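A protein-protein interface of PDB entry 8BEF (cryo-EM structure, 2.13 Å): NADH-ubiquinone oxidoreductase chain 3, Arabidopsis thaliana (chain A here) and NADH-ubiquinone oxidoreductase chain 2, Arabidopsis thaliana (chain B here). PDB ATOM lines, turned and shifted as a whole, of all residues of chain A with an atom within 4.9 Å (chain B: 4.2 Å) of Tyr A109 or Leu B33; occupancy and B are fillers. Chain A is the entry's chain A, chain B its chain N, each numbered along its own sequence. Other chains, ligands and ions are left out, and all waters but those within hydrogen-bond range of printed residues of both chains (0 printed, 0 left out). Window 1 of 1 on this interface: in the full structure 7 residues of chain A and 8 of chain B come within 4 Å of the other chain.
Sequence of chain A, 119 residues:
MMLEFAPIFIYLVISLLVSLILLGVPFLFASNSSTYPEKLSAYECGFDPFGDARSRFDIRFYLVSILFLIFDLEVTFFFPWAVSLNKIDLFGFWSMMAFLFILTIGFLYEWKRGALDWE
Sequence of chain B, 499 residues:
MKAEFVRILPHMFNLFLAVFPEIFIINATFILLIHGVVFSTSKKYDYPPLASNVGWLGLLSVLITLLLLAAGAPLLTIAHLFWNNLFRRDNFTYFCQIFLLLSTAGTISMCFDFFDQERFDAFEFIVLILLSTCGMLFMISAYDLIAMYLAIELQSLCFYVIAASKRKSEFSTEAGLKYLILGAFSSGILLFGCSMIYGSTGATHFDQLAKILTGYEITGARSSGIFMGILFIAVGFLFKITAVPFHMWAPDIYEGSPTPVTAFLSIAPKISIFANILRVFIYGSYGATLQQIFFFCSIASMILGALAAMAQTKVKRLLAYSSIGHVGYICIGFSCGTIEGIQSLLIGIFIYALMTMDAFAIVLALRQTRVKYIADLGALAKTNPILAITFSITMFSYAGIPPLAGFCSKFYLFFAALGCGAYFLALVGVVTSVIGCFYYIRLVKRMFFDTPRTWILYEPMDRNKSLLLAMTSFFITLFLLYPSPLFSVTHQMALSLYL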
ATOM      1  N   ILE A 105     -12.545 -11.555 -22.322  1.00  0.00           N
ATOM      2  CA  ILE A 105     -13.963 -11.235 -22.468  1.00  0.00           C
ATOM      3  C   ILE A 105     -14.464 -10.526 -21.218  1.00  0.00           C
ATOM      4  O   ILE A 105     -15.195  -9.527 -21.296  1.00  0.00           O
ATOM      5  CB  ILE A 105     -14.781 -12.501 -22.771  1.00  0.00           C
ATOM      6  CG1 ILE A 105     -14.576 -12.925 -24.223  1.00  0.00           C
ATOM      7  CG2 ILE A 105     -16.262 -12.270 -22.487  1.00  0.00           C
ATOM      8  CD1 ILE A 105     -15.398 -14.113 -24.611  1.00  0.00           C
ATOM      9  N   GLY A 106     -14.070 -11.025 -20.045  1.00  0.00           N
ATOM     10  CA  GLY A 106     -14.388 -10.307 -18.817  1.00  0.00           C
ATOM     11  C   GLY A 106     -13.842  -8.888 -18.809  1.00  0.00           C
ATOM     12  O   GLY A 106     -14.521  -7.948 -18.379  1.00  0.00           O
ATOM     13  N   PHE A 107     -12.607  -8.718 -19.277  1.00  0.00           N
ATOM     14  CA  PHE A 107     -12.003  -7.389 -19.338  1.00  0.00           C
ATOM     15  C   PHE A 107     -12.778  -6.467 -20.274  1.00  0.00           C
ATOM     16  O   PHE A 107     -12.975  -5.289 -19.966  1.00  0.00           O
ATOM     17  CB  PHE A 107     -10.545  -7.495 -19.783  1.00  0.00           C
ATOM     18  CG  PHE A 107      -9.766  -6.219 -19.627  1.00  0.00           C
ATOM     19  CD1 PHE A 107      -9.644  -5.609 -18.390  1.00  0.00           C
ATOM     20  CD2 PHE A 107      -9.157  -5.629 -20.720  1.00  0.00           C
ATOM     21  CE1 PHE A 107      -8.925  -4.434 -18.247  1.00  0.00           C
ATOM     22  CE2 PHE A 107      -8.439  -4.455 -20.584  1.00  0.00           C
ATOM     23  CZ  PHE A 107      -8.319  -3.859 -19.349  1.00  0.00           C
ATOM     24  N   LEU A 108     -13.204  -6.981 -21.429  1.00  0.00           N
ATOM     25  CA  LEU A 108     -14.013  -6.188 -22.350  1.00  0.00           C
ATOM     26  C   LEU A 108     -15.324  -5.770 -21.700  1.00  0.00           C
ATOM     27  O   LEU A 108     -15.768  -4.625 -21.855  1.00  0.00           O
ATOM     28  CB  LEU A 108     -14.280  -6.977 -23.631  1.00  0.00           C
ATOM     29  CG  LEU A 108     -15.198  -6.335 -24.678  1.00  0.00           C
ATOM     30  CD1 LEU A 108     -14.710  -4.949 -25.084  1.00  0.00           C
ATOM     31  CD2 LEU A 108     -15.335  -7.234 -25.898  1.00  0.00           C
ATOM     32  N   TYR A 109     -15.954  -6.691 -20.968  1.00  0.00           N
ATOM     33  CA  TYR A 109     -17.160  -6.348 -20.220  1.00  0.00           C
ATOM     34  C   TYR A 109     -16.894  -5.207 -19.244  1.00  0.00           C
ATOM     35  O   TYR A 109     -17.677  -4.255 -19.156  1.00  0.00           O
ATOM     36  CB  TYR A 109     -17.686  -7.573 -19.474  1.00  0.00           C
ATOM     37  CG  TYR A 109     -18.882  -7.276 -18.603  1.00  0.00           C
ATOM     38  CD1 TYR A 109     -20.147  -7.122 -19.155  1.00  0.00           C
ATOM     39  CD2 TYR A 109     -18.743  -7.119 -17.234  1.00  0.00           C
ATOM     40  CE1 TYR A 109     -21.243  -6.840 -18.361  1.00  0.00           C
ATOM     41  CE2 TYR A 109     -19.828  -6.837 -16.432  1.00  0.00           C
ATOM     42  CZ  TYR A 109     -21.076  -6.698 -17.000  1.00  0.00           C
ATOM     43  OH  TYR A 109     -22.155  -6.414 -16.201  1.00  0.00           O
ATOM     44  N   GLU A 110     -15.793  -5.290 -18.492  1.00  0.00           N
ATOM     45  CA  GLU A 110     -15.473  -4.219 -17.550  1.00  0.00           C
ATOM     46  C   GLU A 110     -15.229  -2.900 -18.274  1.00  0.00           C
ATOM     47  O   GLU A 110     -15.675  -1.841 -17.819  1.00  0.00           O
ATOM     48  CB  GLU A 110     -14.252  -4.581 -16.708  1.00  0.00           C
ATOM     49  CG  GLU A 110     -14.562  -5.399 -15.476  1.00  0.00           C
ATOM     50  CD  GLU A 110     -13.490  -6.423 -15.214  1.00  0.00           C
ATOM     51  OE1 GLU A 110     -12.599  -6.561 -16.080  1.00  0.00           O
ATOM     52  OE2 GLU A 110     -13.532  -7.086 -14.158  1.00  0.00           O
ATOM     53  N   TRP A 111     -14.515  -2.950 -19.396  1.00  0.00           N
ATOM     54  CA  TRP A 111     -14.201  -1.748 -20.161  1.00  0.00           C
ATOM     55  C   TRP A 111     -15.472  -1.058 -20.641  1.00  0.00           C
ATOM     56  O   TRP A 111     -15.625   0.159 -20.496  1.00  0.00           O
ATOM     57  CB  TRP A 111     -13.308  -2.132 -21.342  1.00  0.00           C
ATOM     58  CG  TRP A 111     -12.715  -1.012 -22.130  1.00  0.00           C
ATOM     59  CD1 TRP A 111     -13.360   0.071 -22.653  1.00  0.00           C
ATOM     60  CD2 TRP A 111     -11.345  -0.890 -22.523  1.00  0.00           C
ATOM     61  NE1 TRP A 111     -12.474   0.864 -23.335  1.00  0.00           N
ATOM     62  CE2 TRP A 111     -11.230   0.294 -23.275  1.00  0.00           C
ATOM     63  CE3 TRP A 111     -10.204  -1.667 -22.309  1.00  0.00           C
ATOM     64  CZ2 TRP A 111     -10.017   0.727 -23.803  1.00  0.00           C
ATOM     65  CZ3 TRP A 111      -9.004  -1.241 -22.842  1.00  0.00           C
ATOM     66  CH2 TRP A 111      -8.918  -0.053 -23.576  1.00  0.00           C
ATOM     67  N   LYS A 112     -16.403  -1.832 -21.203  1.00  0.00           N
ATOM     68  CA  LYS A 112     -17.636  -1.257 -21.732  1.00  0.00           C
ATOM     69  C   LYS A 112     -18.491  -0.651 -20.624  1.00  0.00           C
ATOM     70  O   LYS A 112     -19.113   0.400 -20.812  1.00  0.00           O
ATOM     71  CB  LYS A 112     -18.420  -2.326 -22.491  1.00  0.00           C
ATOM     72  CG  LYS A 112     -17.818  -2.714 -23.827  1.00  0.00           C
ATOM     73  CD  LYS A 112     -17.533  -1.499 -24.688  1.00  0.00           C
ATOM     74  CE  LYS A 112     -18.742  -1.133 -25.532  1.00  0.00           C
ATOM     75  NZ  LYS A 112     -18.979   0.336 -25.587  1.00  0.00           N
ATOM     76  N   ARG A 113     -18.520  -1.292 -19.458  1.00  0.00           N
ATOM     77  CA  ARG A 113     -19.346  -0.850 -18.342  1.00  0.00           C
ATOM     78  C   ARG A 113     -18.787   0.370 -17.618  1.00  0.00           C
ATOM     79  O   ARG A 113     -19.448   0.880 -16.711  1.00  0.00           O
ATOM     80  CB  ARG A 113     -19.536  -1.994 -17.343  1.00  0.00           C
ATOM     81  CG  ARG A 113     -20.581  -3.011 -17.760  1.00  0.00           C
ATOM     82  CD  ARG A 113     -21.955  -2.581 -17.294  1.00  0.00           C
ATOM     83  NE  ARG A 113     -23.013  -3.459 -17.771  1.00  0.00           N
ATOM     84  CZ  ARG A 113     -23.900  -3.129 -18.699  1.00  0.00           C
ATOM     85  NH1 ARG A 113     -23.840  -1.970 -19.330  1.00  0.00           N
ATOM     86  NH2 ARG A 113     -24.879  -3.979 -18.991  1.00  0.00           N
ATOM     87  N   THR B  29     -22.859 -18.406 -24.518  1.00  0.00           N
ATOM     88  CA  THR B  29     -22.910 -17.505 -23.374  1.00  0.00           C
ATOM     89  C   THR B  29     -21.971 -16.321 -23.567  1.00  0.00           C
ATOM     90  O   THR B  29     -22.326 -15.179 -23.253  1.00  0.00           O
ATOM     91  CB  THR B  29     -22.568 -18.276 -22.098  1.00  0.00           C
ATOM     92  OG1 THR B  29     -23.512 -19.341 -21.921  1.00  0.00           O
ATOM     93  CG2 THR B  29     -22.606 -17.366 -20.888  1.00  0.00           C
ATOM     94  N   PHE B  30     -20.772 -16.574 -24.091  1.00  0.00           N
ATOM     95  CA  PHE B  30     -19.851 -15.475 -24.377  1.00  0.00           C
ATOM     96  C   PHE B  30     -20.432 -14.531 -25.426  1.00  0.00           C
ATOM     97  O   PHE B  30     -20.342 -13.300 -25.294  1.00  0.00           O
ATOM     98  CB  PHE B  30     -18.505 -16.027 -24.842  1.00  0.00           C
ATOM     99  CG  PHE B  30     -17.745 -16.758 -23.772  1.00  0.00           C
ATOM    100  CD1 PHE B  30     -18.111 -16.651 -22.440  1.00  0.00           C
ATOM    101  CD2 PHE B  30     -16.666 -17.562 -24.100  1.00  0.00           C
ATOM    102  CE1 PHE B  30     -17.415 -17.331 -21.456  1.00  0.00           C
ATOM    103  CE2 PHE B  30     -15.966 -18.241 -23.119  1.00  0.00           C
ATOM    104  CZ  PHE B  30     -16.341 -18.124 -21.798  1.00  0.00           C
ATOM    105  N   ILE B  31     -21.034 -15.096 -26.475  1.00  0.00           N
ATOM    106  CA  ILE B  31     -21.639 -14.280 -27.525  1.00  0.00           C
ATOM    107  C   ILE B  31     -22.728 -13.390 -26.942  1.00  0.00           C
ATOM    108  O   ILE B  31     -22.809 -12.196 -27.258  1.00  0.00           O
ATOM    109  CB  ILE B  31     -22.182 -15.178 -28.653  1.00  0.00           C
ATOM    110  CG1 ILE B  31     -21.028 -15.759 -29.472  1.00  0.00           C
ATOM    111  CG2 ILE B  31     -23.151 -14.410 -29.548  1.00  0.00           C
ATOM    112  CD1 ILE B  31     -21.431 -16.888 -30.380  1.00  0.00           C
ATOM    113  N   LEU B  32     -23.579 -13.954 -26.083  1.00  0.00           N
ATOM    114  CA  LEU B  32     -24.653 -13.169 -25.482  1.00  0.00           C
ATOM    115  C   LEU B  32     -24.111 -12.102 -24.540  1.00  0.00           C
ATOM    116  O   LEU B  32     -24.647 -10.993 -24.488  1.00  0.00           O
ATOM    117  CB  LEU B  32     -25.642 -14.082 -24.760  1.00  0.00           C
ATOM    118  CG  LEU B  32     -26.326 -15.082 -25.692  1.00  0.00           C
ATOM    119  CD1 LEU B  32     -27.133 -16.119 -24.919  1.00  0.00           C
ATOM    120  CD2 LEU B  32     -27.188 -14.329 -26.684  1.00  0.00           C
ATOM    121  N   LEU B  33     -23.055 -12.414 -23.786  1.00  0.00           N
ATOM    122  CA  LEU B  33     -22.438 -11.397 -22.938  1.00  0.00           C
ATOM    123  C   LEU B  33     -21.975 -10.207 -23.769  1.00  0.00           C
ATOM    124  O   LEU B  33     -22.254  -9.048 -23.432  1.00  0.00           O
ATOM    125  CB  LEU B  33     -21.262 -11.997 -22.164  1.00  0.00           C
ATOM    126  CG  LEU B  33     -20.562 -11.061 -21.173  1.00  0.00           C
ATOM    127  CD1 LEU B  33     -21.551 -10.503 -20.162  1.00  0.00           C
ATOM    128  CD2 LEU B  33     -19.404 -11.759 -20.471  1.00  0.00           C
ATOM    129  N   ILE B  34     -21.284 -10.482 -24.877  1.00  0.00           N
ATOM    130  CA  ILE B  34     -20.772  -9.404 -25.720  1.00  0.00           C
ATOM    131  C   ILE B  34     -21.920  -8.613 -26.341  1.00  0.00           C
ATOM    132  O   ILE B  34     -21.919  -7.378 -26.326  1.00  0.00           O
ATOM    133  CB  ILE B  34     -19.824  -9.967 -26.795  1.00  0.00           C
ATOM    134  CG1 ILE B  34     -18.599 -10.606 -26.141  1.00  0.00           C
ATOM    135  CG2 ILE B  34     -19.391  -8.871 -27.745  1.00  0.00           C
ATOM    136  CD1 ILE B  34     -17.952 -11.681 -26.975  1.00  0.00           C
ATOM    137  N   HIS B  35     -22.909  -9.315 -26.901  1.00  0.00           N
ATOM    138  CA  HIS B  35     -24.084  -8.665 -27.483  1.00  0.00           C
ATOM    139  C   HIS B  35     -24.759  -7.736 -26.476  1.00  0.00           C
ATOM    140  O   HIS B  35     -25.013  -6.554 -26.760  1.00  0.00           O
ATOM    141  CB  HIS B  35     -25.051  -9.752 -27.973  1.00  0.00           C
ATOM    142  CG  HIS B  35     -26.412  -9.254 -28.349  1.00  0.00           C
ATOM    143  ND1 HIS B  35     -26.725  -8.832 -29.623  1.00  0.00           N
ATOM    144  CD2 HIS B  35     -27.553  -9.146 -27.627  1.00  0.00           C
ATOM    145  CE1 HIS B  35     -27.993  -8.468 -29.666  1.00  0.00           C
ATOM    146  NE2 HIS B  35     -28.520  -8.651 -28.468  1.00  0.00           N
ATOM    147  N   GLY B  36     -25.026  -8.260 -25.277  1.00  0.00           N
ATOM    148  CA  GLY B  36     -25.699  -7.476 -24.261  1.00  0.00           C
ATOM    149  C   GLY B  36     -24.912  -6.247 -23.856  1.00  0.00           C
ATOM    150  O   GLY B  36     -25.463  -5.151 -23.768  1.00  0.00           O
ATOM    151  N   VAL B  37     -23.608  -6.409 -23.613  1.00  0.00           N
ATOM    152  CA  VAL B  37     -22.840  -5.260 -23.145  1.00  0.00           C
ATOM    153  C   VAL B  37     -22.658  -4.230 -24.257  1.00  0.00           C
ATOM    154  O   VAL B  37     -22.603  -3.026 -23.983  1.00  0.00           O
ATOM    155  CB  VAL B  37     -21.491  -5.695 -22.540  1.00  0.00           C
ATOM    156  CG1 VAL B  37     -20.440  -5.925 -23.618  1.00  0.00           C
ATOM    157  CG2 VAL B  37     -21.020  -4.654 -21.540  1.00  0.00           C
ATOM    158  N   PHE B 123     -29.474  -7.922 -18.337  1.00  0.00           N
ATOM    159  CA  PHE B 123     -29.252  -9.137 -19.113  1.00  0.00           C
ATOM    160  C   PHE B 123     -28.219 -10.049 -18.466  1.00  0.00           C
ATOM    161  O   PHE B 123     -28.179 -11.242 -18.783  1.00  0.00           O
ATOM    162  CB  PHE B 123     -28.805  -8.791 -20.534  1.00  0.00           C
ATOM    163  CG  PHE B 123     -27.381  -8.326 -20.621  1.00  0.00           C
ATOM    164  CD1 PHE B 123     -26.348  -9.230 -20.826  1.00  0.00           C
ATOM    165  CD2 PHE B 123     -27.072  -6.984 -20.491  1.00  0.00           C
ATOM    166  CE1 PHE B 123     -25.041  -8.804 -20.898  1.00  0.00           C
ATOM    167  CE2 PHE B 123     -25.765  -6.553 -20.562  1.00  0.00           C
ATOM    168  CZ  PHE B 123     -24.748  -7.460 -20.763  1.00  0.00           C
ATOM    169  N   GLU B 124     -27.368  -9.508 -17.591  1.00  0.00           N
ATOM    170  CA  GLU B 124     -26.351 -10.321 -16.932  1.00  0.00           C
ATOM    171  C   GLU B 124     -26.978 -11.445 -16.119  1.00  0.00           C
ATOM    172  O   GLU B 124     -26.331 -12.464 -15.866  1.00  0.00           O
ATOM    173  CB  GLU B 124     -25.473  -9.440 -16.043  1.00  0.00           C
ATOM    174  CG  GLU B 124     -24.559  -8.494 -16.813  1.00  0.00           C
ATOM    175  CD  GLU B 124     -25.190  -7.133 -17.080  1.00  0.00           C
ATOM    176  OE1 GLU B 124     -26.433  -7.039 -17.126  1.00  0.00           O
ATOM    177  OE2 GLU B 124     -24.435  -6.155 -17.252  1.00  0.00           O
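Of the 11 printed residues of chain B, 5 touch a printed residue of chain A.
The side-chain hydroxyl (OH) of Tyr A109 sits at hydrogen-bond distance from the side-chain carboxylate (OE2) of Glu B124, at 2.5 Å.
The side-chain carboxylate (OE2) of Glu B124 is in salt-bridge range of the guanidinium group (NH2) of Arg A113, at 2.8 Å.
NE of Arg A113 lies within hydrogen-bond range of OH of Tyr A109.
Tyr A109 touches just these residues of chain B: Leu B33, Val B37 and Glu B124.
Leu B33 touches just these residues of chain A: Ile A105 (3.8 Å) and Tyr A109 (3.8 Å).
Printed residues of chain B within 4 Å of Arg A113: Phe B123 (3.1 Å) and Glu B124 (2.8 Å).
Of the printed residues of chain A, Phe B30 touches Ile A105 (3.6 Å).
The nearest printed residue of chain A that does not touch Leu B33 is Gly A106 (5.4 Å).
CD1 of Ile A105 touches CG of Phe B30 (3.6 Å).
Leu B33 touches Ile A105.
CD1 of Tyr A109 touches CD1 of Leu B33 (3.8 Å).
Tyr A109 touches Val B37 (CD1 to CG2, 3.5 Å).
CB of Lys A112 touches CG2 of Val B37, at 3.6 Å.
Phe B123 touches Arg A113 (CE2 to NH2, 3.1 Å).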
